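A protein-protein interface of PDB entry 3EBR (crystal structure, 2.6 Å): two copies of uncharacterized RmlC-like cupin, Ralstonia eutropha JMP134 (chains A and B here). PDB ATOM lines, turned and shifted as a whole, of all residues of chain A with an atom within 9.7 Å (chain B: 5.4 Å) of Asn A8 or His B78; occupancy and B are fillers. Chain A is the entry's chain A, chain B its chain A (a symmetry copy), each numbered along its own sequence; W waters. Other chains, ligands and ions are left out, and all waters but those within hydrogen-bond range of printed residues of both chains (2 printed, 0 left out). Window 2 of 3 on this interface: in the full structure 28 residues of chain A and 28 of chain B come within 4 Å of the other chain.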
ATOM      1  N   LEU A   3      -8.846   1.118 -11.647  1.00  0.00           N
ATOM      2  CA  LEU A   3      -8.707   2.184 -12.683  1.00  0.00           C
ATOM      3  C   LEU A   3      -9.327   1.963 -14.068  1.00  0.00           C
ATOM      4  O   LEU A   3      -9.882   2.916 -14.619  1.00  0.00           O
ATOM      5  CB  LEU A   3      -7.230   2.513 -12.941  1.00  0.00           C
ATOM      6  N   PHE A   4      -9.262   0.733 -14.601  1.00  0.00           N
ATOM      7  CA  PHE A   4      -9.793   0.432 -15.963  1.00  0.00           C
ATOM      8  C   PHE A   4     -11.300   0.714 -16.127  1.00  0.00           C
ATOM      9  O   PHE A   4     -11.762   0.971 -17.248  1.00  0.00           O
ATOM     10  CB  PHE A   4      -9.474  -1.014 -16.416  1.00  0.00           C
ATOM     11  CG  PHE A   4     -10.411  -2.081 -15.876  1.00  0.00           C
ATOM     12  CD1 PHE A   4     -11.585  -2.412 -16.581  1.00  0.00           C
ATOM     13  CD2 PHE A   4     -10.110  -2.794 -14.719  1.00  0.00           C
ATOM     14  CE1 PHE A   4     -12.456  -3.395 -16.122  1.00  0.00           C
ATOM     15  CE2 PHE A   4     -10.979  -3.790 -14.263  1.00  0.00           C
ATOM     16  CZ  PHE A   4     -12.154  -4.084 -14.963  1.00  0.00           C
ATOM     17  N   GLU A   5     -12.045   0.604 -15.020  1.00  0.00           N
ATOM     18  CA  GLU A   5     -13.482   0.898 -14.967  1.00  0.00           C
ATOM     19  C   GLU A   5     -13.751   2.387 -15.308  1.00  0.00           C
ATOM     20  O   GLU A   5     -14.774   2.697 -15.925  1.00  0.00           O
ATOM     21  CB  GLU A   5     -14.067   0.500 -13.598  1.00  0.00           C
ATOM     22  CG  GLU A   5     -14.021  -1.034 -13.321  1.00  0.00           C
ATOM     23  CD  GLU A   5     -14.490  -1.449 -11.925  1.00  0.00           C
ATOM     24  OE1 GLU A   5     -14.613  -0.588 -11.027  1.00  0.00           O
ATOM     25  OE2 GLU A   5     -14.708  -2.663 -11.716  1.00  0.00           O
ATOM     26  N   SER A   6     -12.827   3.280 -14.925  1.00  0.00           N
ATOM     27  CA  SER A   6     -12.910   4.717 -15.213  1.00  0.00           C
ATOM     28  C   SER A   6     -12.242   5.145 -16.551  1.00  0.00           C
ATOM     29  O   SER A   6     -12.582   6.222 -17.050  1.00  0.00           O
ATOM     30  CB  SER A   6     -12.296   5.521 -14.057  1.00  0.00           C
ATOM     31  N   ILE A   7     -11.311   4.349 -17.117  1.00  0.00           N
ATOM     32  CA  ILE A   7     -10.620   4.703 -18.402  1.00  0.00           C
ATOM     33  C   ILE A   7     -11.524   4.658 -19.649  1.00  0.00           C
ATOM     34  O   ILE A   7     -12.195   3.653 -19.895  1.00  0.00           O
ATOM     35  CB  ILE A   7      -9.330   3.858 -18.695  1.00  0.00           C
ATOM     36  CG1 ILE A   7      -8.092   4.440 -18.013  1.00  0.00           C
ATOM     37  CG2 ILE A   7      -8.970   3.889 -20.175  1.00  0.00           C
ATOM     38  CD1 ILE A   7      -8.172   4.661 -16.531  1.00  0.00           C
ATOM     39  N   ASN A   8     -11.517   5.753 -20.424  1.00  0.00           N
ATOM     40  CA  ASN A   8     -12.316   5.880 -21.642  1.00  0.00           C
ATOM     41  C   ASN A   8     -11.776   7.021 -22.538  1.00  0.00           C
ATOM     42  O   ASN A   8     -10.887   7.787 -22.118  1.00  0.00           O
ATOM     43  CB  ASN A   8     -13.795   6.120 -21.251  1.00  0.00           C
ATOM     44  CG  ASN A   8     -14.797   5.775 -22.357  1.00  0.00           C
ATOM     45  OD1 ASN A   8     -14.437   5.323 -23.457  1.00  0.00           O
ATOM     46  ND2 ASN A   8     -16.075   5.983 -22.053  1.00  0.00           N
ATOM     47  N   THR A   9     -12.262   7.095 -23.779  1.00  0.00           N
ATOM     48  CA  THR A   9     -11.887   8.142 -24.721  1.00  0.00           C
ATOM     49  C   THR A   9     -12.443   9.489 -24.260  1.00  0.00           C
ATOM     50  O   THR A   9     -13.663   9.632 -24.081  1.00  0.00           O
ATOM     51  CB  THR A   9     -12.408   7.824 -26.116  1.00  0.00           C
ATOM     52  OG1 THR A   9     -11.813   6.594 -26.519  1.00  0.00           O
ATOM     53  CG2 THR A   9     -12.057   8.926 -27.122  1.00  0.00           C
ATOM     54  N   GLY A  10     -11.529  10.437 -24.044  1.00  0.00           N
ATOM     55  CA  GLY A  10     -11.838  11.789 -23.606  1.00  0.00           C
ATOM     56  C   GLY A  10     -11.564  12.812 -24.690  1.00  0.00           C
ATOM     57  O   GLY A  10     -10.984  12.513 -25.741  1.00  0.00           O
ATOM     58  N   CYS A  11     -11.990  14.033 -24.399  1.00  0.00           N
ATOM     59  CA  CYS A  11     -11.845  15.165 -25.286  1.00  0.00           C
ATOM     60  C   CYS A  11     -11.778  16.438 -24.474  1.00  0.00           C
ATOM     61  O   CYS A  11     -12.671  16.673 -23.666  1.00  0.00           O
ATOM     62  CB  CYS A  11     -13.043  15.241 -26.219  1.00  0.00           C
ATOM     63  SG  CYS A  11     -13.031  16.689 -27.278  1.00  0.00           S
ATOM     64  N   LYS A  35      -2.732  17.182 -21.976  1.00  0.00           N
ATOM     65  CA  LYS A  35      -2.536  15.923 -21.285  1.00  0.00           C
ATOM     66  C   LYS A  35      -1.177  15.981 -20.595  1.00  0.00           C
ATOM     67  O   LYS A  35      -0.268  16.587 -21.127  1.00  0.00           O
ATOM     68  CB  LYS A  35      -2.585  14.774 -22.298  1.00  0.00           C
ATOM     69  CG  LYS A  35      -3.152  13.460 -21.781  1.00  0.00           C
ATOM     70  CD  LYS A  35      -4.674  13.623 -21.622  1.00  0.00           C
ATOM     71  CE  LYS A  35      -5.350  12.415 -21.096  1.00  0.00           C
ATOM     72  NZ  LYS A  35      -6.770  12.749 -20.769  1.00  0.00           N
ATOM     73  N   THR A 156      -5.223  11.609 -15.718  1.00  0.00           N
ATOM     74  CA  THR A 156      -5.993  10.425 -16.178  1.00  0.00           C
ATOM     75  C   THR A 156      -6.413  10.517 -17.643  1.00  0.00           C
ATOM     76  O   THR A 156      -6.437  11.611 -18.226  1.00  0.00           O
ATOM     77  CB  THR A 156      -7.308  10.169 -15.371  1.00  0.00           C
ATOM     78  OG1 THR A 156      -8.147  11.332 -15.426  1.00  0.00           O
ATOM     79  CG2 THR A 156      -7.016   9.853 -13.954  1.00  0.00           C
ATOM     80  N   PHE A 157      -6.757   9.341 -18.191  1.00  0.00           N
ATOM     81  CA  PHE A 157      -7.237   9.131 -19.557  1.00  0.00           C
ATOM     82  C   PHE A 157      -8.701   8.747 -19.396  1.00  0.00           C
ATOM     83  O   PHE A 157      -9.021   7.564 -19.296  1.00  0.00           O
ATOM     84  CB  PHE A 157      -6.423   8.047 -20.265  1.00  0.00           C
ATOM     85  CG  PHE A 157      -4.978   8.398 -20.424  1.00  0.00           C
ATOM     86  CD1 PHE A 157      -4.054   8.058 -19.438  1.00  0.00           C
ATOM     87  CD2 PHE A 157      -4.539   9.075 -21.552  1.00  0.00           C
ATOM     88  CE1 PHE A 157      -2.716   8.395 -19.576  1.00  0.00           C
ATOM     89  CE2 PHE A 157      -3.203   9.423 -21.696  1.00  0.00           C
ATOM     90  CZ  PHE A 157      -2.290   9.081 -20.711  1.00  0.00           C
ATOM     91  N   GLU A 158      -9.577   9.754 -19.359  1.00  0.00           N
ATOM     92  CA  GLU A 158     -11.011   9.552 -19.127  1.00  0.00           C
ATOM     93  C   GLU A 158     -11.881  10.624 -19.779  1.00  0.00           C
ATOM     94  O   GLU A 158     -12.890  10.306 -20.413  1.00  0.00           O
ATOM     95  CB  GLU A 158     -11.190   9.499 -17.604  1.00  0.00           C
ATOM     96  CG  GLU A 158     -12.602   9.446 -17.034  1.00  0.00           C
ATOM     97  CD  GLU A 158     -12.614   9.214 -15.517  1.00  0.00           C
ATOM     98  OE1 GLU A 158     -11.553   9.344 -14.857  1.00  0.00           O
ATOM     99  OE2 GLU A 158     -13.702   8.910 -14.977  1.00  0.00           O
ATOM    100  N   ARG B  74     -17.484  14.244 -34.091  1.00  0.00           N
ATOM    101  CA  ARG B  74     -17.785  13.514 -32.868  1.00  0.00           C
ATOM    102  C   ARG B  74     -17.920  12.032 -33.126  1.00  0.00           C
ATOM    103  O   ARG B  74     -17.924  11.602 -34.280  1.00  0.00           O
ATOM    104  CB  ARG B  74     -19.099  14.036 -32.282  1.00  0.00           C
ATOM    105  CG  ARG B  74     -20.279  14.074 -33.289  1.00  0.00           C
ATOM    106  CD  ARG B  74     -21.526  14.643 -32.658  1.00  0.00           C
ATOM    107  NE  ARG B  74     -22.260  13.649 -31.878  1.00  0.00           N
ATOM    108  CZ  ARG B  74     -23.302  12.921 -32.303  1.00  0.00           C
ATOM    109  NH1 ARG B  74     -23.827  13.043 -33.538  1.00  0.00           N
ATOM    110  NH2 ARG B  74     -23.856  12.051 -31.454  1.00  0.00           N
ATOM    111  N   TYR B  75     -18.006  11.270 -32.039  1.00  0.00           N
ATOM    112  CA  TYR B  75     -18.228   9.839 -32.083  1.00  0.00           C
ATOM    113  C   TYR B  75     -19.672   9.645 -31.685  1.00  0.00           C
ATOM    114  O   TYR B  75     -20.135  10.315 -30.754  1.00  0.00           O
ATOM    115  CB  TYR B  75     -17.325   9.061 -31.125  1.00  0.00           C
ATOM    116  CG  TYR B  75     -15.856   9.150 -31.442  1.00  0.00           C
ATOM    117  CD1 TYR B  75     -15.375   8.709 -32.675  1.00  0.00           C
ATOM    118  CD2 TYR B  75     -14.929   9.598 -30.499  1.00  0.00           C
ATOM    119  CE1 TYR B  75     -14.024   8.740 -32.986  1.00  0.00           C
ATOM    120  CE2 TYR B  75     -13.550   9.638 -30.805  1.00  0.00           C
ATOM    121  CZ  TYR B  75     -13.116   9.194 -32.047  1.00  0.00           C
ATOM    122  OH  TYR B  75     -11.796   9.259 -32.389  1.00  0.00           O
ATOM    123  N   LYS B  76     -20.388   8.745 -32.376  1.00  0.00           N
ATOM    124  CA  LYS B  76     -21.795   8.427 -32.050  1.00  0.00           C
ATOM    125  C   LYS B  76     -21.964   7.822 -30.642  1.00  0.00           C
ATOM    126  O   LYS B  76     -23.022   7.957 -30.041  1.00  0.00           O
ATOM    127  CB  LYS B  76     -22.414   7.438 -33.053  1.00  0.00           C
ATOM    128  CG  LYS B  76     -22.560   7.913 -34.489  1.00  0.00           C
ATOM    129  CD  LYS B  76     -23.315   6.873 -35.351  1.00  0.00           C
ATOM    130  N   GLU B  77     -20.914   7.175 -30.133  1.00  0.00           N
ATOM    131  CA  GLU B  77     -20.895   6.532 -28.826  1.00  0.00           C
ATOM    132  C   GLU B  77     -20.653   7.499 -27.640  1.00  0.00           C
ATOM    133  O   GLU B  77     -20.832   7.072 -26.498  1.00  0.00           O
ATOM    134  CB  GLU B  77     -19.817   5.413 -28.789  1.00  0.00           C
ATOM    135  CG  GLU B  77     -19.946   4.224 -29.811  1.00  0.00           C
ATOM    136  CD  GLU B  77     -19.569   4.529 -31.271  1.00  0.00           C
ATOM    137  OE1 GLU B  77     -19.151   5.665 -31.577  1.00  0.00           O
ATOM    138  OE2 GLU B  77     -19.673   3.624 -32.123  1.00  0.00           O
ATOM    139  N   HIS B  78     -20.241   8.755 -27.896  1.00  0.00           N
ATOM    140  CA  HIS B  78     -19.972   9.767 -26.848  1.00  0.00           C
ATOM    141  C   HIS B  78     -20.828  11.029 -27.019  1.00  0.00           C
ATOM    142  O   HIS B  78     -21.251  11.341 -28.131  1.00  0.00           O
ATOM    143  CB  HIS B  78     -18.494  10.123 -26.850  1.00  0.00           C
ATOM    144  CG  HIS B  78     -17.604   8.963 -26.536  1.00  0.00           C
ATOM    145  ND1 HIS B  78     -17.218   8.653 -25.252  1.00  0.00           N
ATOM    146  CD2 HIS B  78     -17.037   8.029 -27.336  1.00  0.00           C
ATOM    147  CE1 HIS B  78     -16.444   7.584 -25.273  1.00  0.00           C
ATOM    148  NE2 HIS B  78     -16.319   7.184 -26.525  1.00  0.00           N
ATOM    149  N   ASP B  79     -21.043  11.754 -25.913  1.00  0.00           N
ATOM    150  CA  ASP B  79     -21.889  12.972 -25.881  1.00  0.00           C
ATOM    151  C   ASP B  79     -21.194  14.340 -26.112  1.00  0.00           C
ATOM    152  O   ASP B  79     -21.849  15.381 -26.006  1.00  0.00           O
ATOM    153  CB  ASP B  79     -22.643  13.006 -24.538  1.00  0.00           C
ATOM    154  N   TRP B  80     -19.917  14.328 -26.489  1.00  0.00           N
ATOM    155  CA  TRP B  80     -19.116  15.549 -26.726  1.00  0.00           C
ATOM    156  C   TRP B  80     -18.810  15.739 -28.206  1.00  0.00           C
ATOM    157  O   TRP B  80     -18.892  14.785 -28.983  1.00  0.00           O
ATOM    158  CB  TRP B  80     -17.805  15.537 -25.900  1.00  0.00           C
ATOM    159  CG  TRP B  80     -16.991  14.270 -25.991  1.00  0.00           C
ATOM    160  CD1 TRP B  80     -16.973  13.249 -25.076  1.00  0.00           C
ATOM    161  CD2 TRP B  80     -16.130  13.857 -27.068  1.00  0.00           C
ATOM    162  NE1 TRP B  80     -16.135  12.241 -25.503  1.00  0.00           N
ATOM    163  CE2 TRP B  80     -15.608  12.587 -26.720  1.00  0.00           C
ATOM    164  CE3 TRP B  80     -15.743  14.434 -28.290  1.00  0.00           C
ATOM    165  CZ2 TRP B  80     -14.736  11.888 -27.550  1.00  0.00           C
ATOM    166  CZ3 TRP B  80     -14.870  13.734 -29.111  1.00  0.00           C
ATOM    167  CH2 TRP B  80     -14.377  12.476 -28.736  1.00  0.00           C
ATOM    168  N   TYR B  89      -8.180  11.927 -27.147  1.00  0.00           N
ATOM    169  CA  TYR B  89      -7.260  10.833 -26.850  1.00  0.00           C
ATOM    170  C   TYR B  89      -8.067   9.535 -26.737  1.00  0.00           C
ATOM    171  O   TYR B  89      -8.706   9.307 -25.711  1.00  0.00           O
ATOM    172  CB  TYR B  89      -6.476  11.115 -25.555  1.00  0.00           C
ATOM    173  CG  TYR B  89      -5.196  10.278 -25.378  1.00  0.00           C
ATOM    174  CD1 TYR B  89      -5.237   8.905 -25.043  1.00  0.00           C
ATOM    175  CD2 TYR B  89      -3.930  10.881 -25.508  1.00  0.00           C
ATOM    176  CE1 TYR B  89      -4.055   8.159 -24.881  1.00  0.00           C
ATOM    177  CE2 TYR B  89      -2.751  10.145 -25.344  1.00  0.00           C
ATOM    178  CZ  TYR B  89      -2.822   8.786 -25.041  1.00  0.00           C
ATOM    179  OH  TYR B  89      -1.650   8.091 -24.873  1.00  0.00           O
ATOM    180  N   THR B  91      -8.380   5.559 -26.230  1.00  0.00           N
ATOM    181  CA  THR B  91      -7.610   4.509 -25.522  1.00  0.00           C
ATOM    182  C   THR B  91      -7.794   3.127 -26.176  1.00  0.00           C
ATOM    183  O   THR B  91      -8.745   2.910 -26.903  1.00  0.00           O
ATOM    184  CB  THR B  91      -7.982   4.448 -24.038  1.00  0.00           C
ATOM    185  OG1 THR B  91      -9.401   4.327 -23.908  1.00  0.00           O
ATOM    186  CG2 THR B  91      -7.538   5.710 -23.333  1.00  0.00           C
ATOM    187  N   THR B  94     -11.111  -0.098 -27.950  1.00  0.00           N
ATOM    188  CA  THR B  94     -12.400   0.592 -27.873  1.00  0.00           C
ATOM    189  C   THR B  94     -12.965   0.748 -29.288  1.00  0.00           C
ATOM    190  O   THR B  94     -12.202   0.765 -30.269  1.00  0.00           O
ATOM    191  CB  THR B  94     -12.258   1.937 -27.155  1.00  0.00           C
ATOM    192  OG1 THR B  94     -11.275   2.727 -27.824  1.00  0.00           O
ATOM    193  CG2 THR B  94     -11.826   1.712 -25.707  1.00  0.00           C
ATOM    194  N   HIS B  96     -15.500   2.940 -31.992  1.00  0.00           N
ATOM    195  CA  HIS B  96     -15.984   4.281 -32.321  1.00  0.00           C
ATOM    196  C   HIS B  96     -16.476   4.446 -33.748  1.00  0.00           C
ATOM    197  O   HIS B  96     -15.872   3.892 -34.664  1.00  0.00           O
ATOM    198  CB  HIS B  96     -14.856   5.281 -32.140  1.00  0.00           C
ATOM    199  CG  HIS B  96     -14.431   5.454 -30.726  1.00  0.00           C
ATOM    200  ND1 HIS B  96     -13.260   4.920 -30.242  1.00  0.00           N
ATOM    201  CD2 HIS B  96     -15.060   6.020 -29.668  1.00  0.00           C
ATOM    202  CE1 HIS B  96     -13.162   5.192 -28.955  1.00  0.00           C
ATOM    203  NE2 HIS B  96     -14.241   5.859 -28.579  1.00  0.00           N
HETATM  204  O   HOH W   1     -14.726  14.037 -22.921  1.00  0.00           O
HETATM  205  O   HOH W   2      -8.834   9.633 -22.896  1.00  0.00           O
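No position is printed for both chains.
Of the 11 pairs that touch across the chains among the printed residues, none has its exchanged pair printed and touching as well.
Water W2 lies within hydrogen-bond range of O of Tyr B89 (2.8 Å), O of Asn A8 (2.9 Å) and N of Gly A10 (3.0 Å).
Water W1 bridges N of Cys A11 (3.1 Å) and NE1 of Trp B80 (3.4 Å).
NE2 of His B96 sits close to OG1 of Thr A9 (3.3 Å).
The backbone carbonyl oxygen (O) of Gly A10 is in hydrogen-bond range of the backbone NH (N) of Tyr B89 (3.2 Å).
Printed residues of chain B that touch a printed residue of chain A: His B78, Trp B80, Tyr B89, Thr B91 and His B96.
Hydrophobic or aromatic side chains of chain B within 4 Å of the printed part of chain A: His B78, Trp B80, Tyr B89 and His B96.
Of the 13 printed residues of chain A, 6 touch a printed residue of chain B.
Hydrophobic or aromatic side chains of chain A within 4 Å of the printed part of chain B: Ile A7 and Phe A157.
Among the printed residues, 11 pairs touch across the chains.
Among the printed residues, no Asp or Glu carboxylate lies within 4 Å of a Lys or Arg side-chain nitrogen of the other chain.
Among the printed residues, pairs that only touch across the chains: Ile A7 with Thr B91, Asn A8 with His B78, Asn A8 with Thr B91, Thr A9 with His B78, Thr A9 with Trp B80, Thr A9 with Tyr B89, Thr A9 with Thr B91, Cys A11 with Trp B80 and Phe A157 with Tyr B89.
N of Asn A8 sits at hydrogen-bond distance from O of Phe A157, at 3.3 Å.
NE2 of His B78 lies within hydrogen-bond range of NE2 of His B96 (3.2 Å).
The backbone carbonyl oxygen (O) of Thr B91 sits at hydrogen-bond distance from the side-chain hydroxyl (OG1) of Thr B94 (2.7 Å).
Asn A8 touches two residues of chain B.
Printed residues of chain B within 4 Å of Gly A10: Tyr B89.
Of the printed residues of chain B, Cys A11 touches Trp B80 (3.5 Å).
Of the printed residues of chain B, Phe A157 touches Tyr B89 (3.4 Å).
Lys B76 touches none of the printed residues of chain A.
Of chain A, only Asn A8 (3.5 Å) and Thr A9 (3.7 Å) come within 4 Å of His B78.
No residue of chain A comes within 4 Å of Asp B79.
Of chain A, only Thr A9 and Cys A11 come within 4 Å of Trp B80.
Of the printed residues of chain A, Tyr B89 touches Thr A9 (3.5 Å), Gly A10 (3.2 Å) and Phe A157 (3.4 Å).
The nearest printed residue of chain B that does not touch Gly A10 is Trp B80 (4.2 Å).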
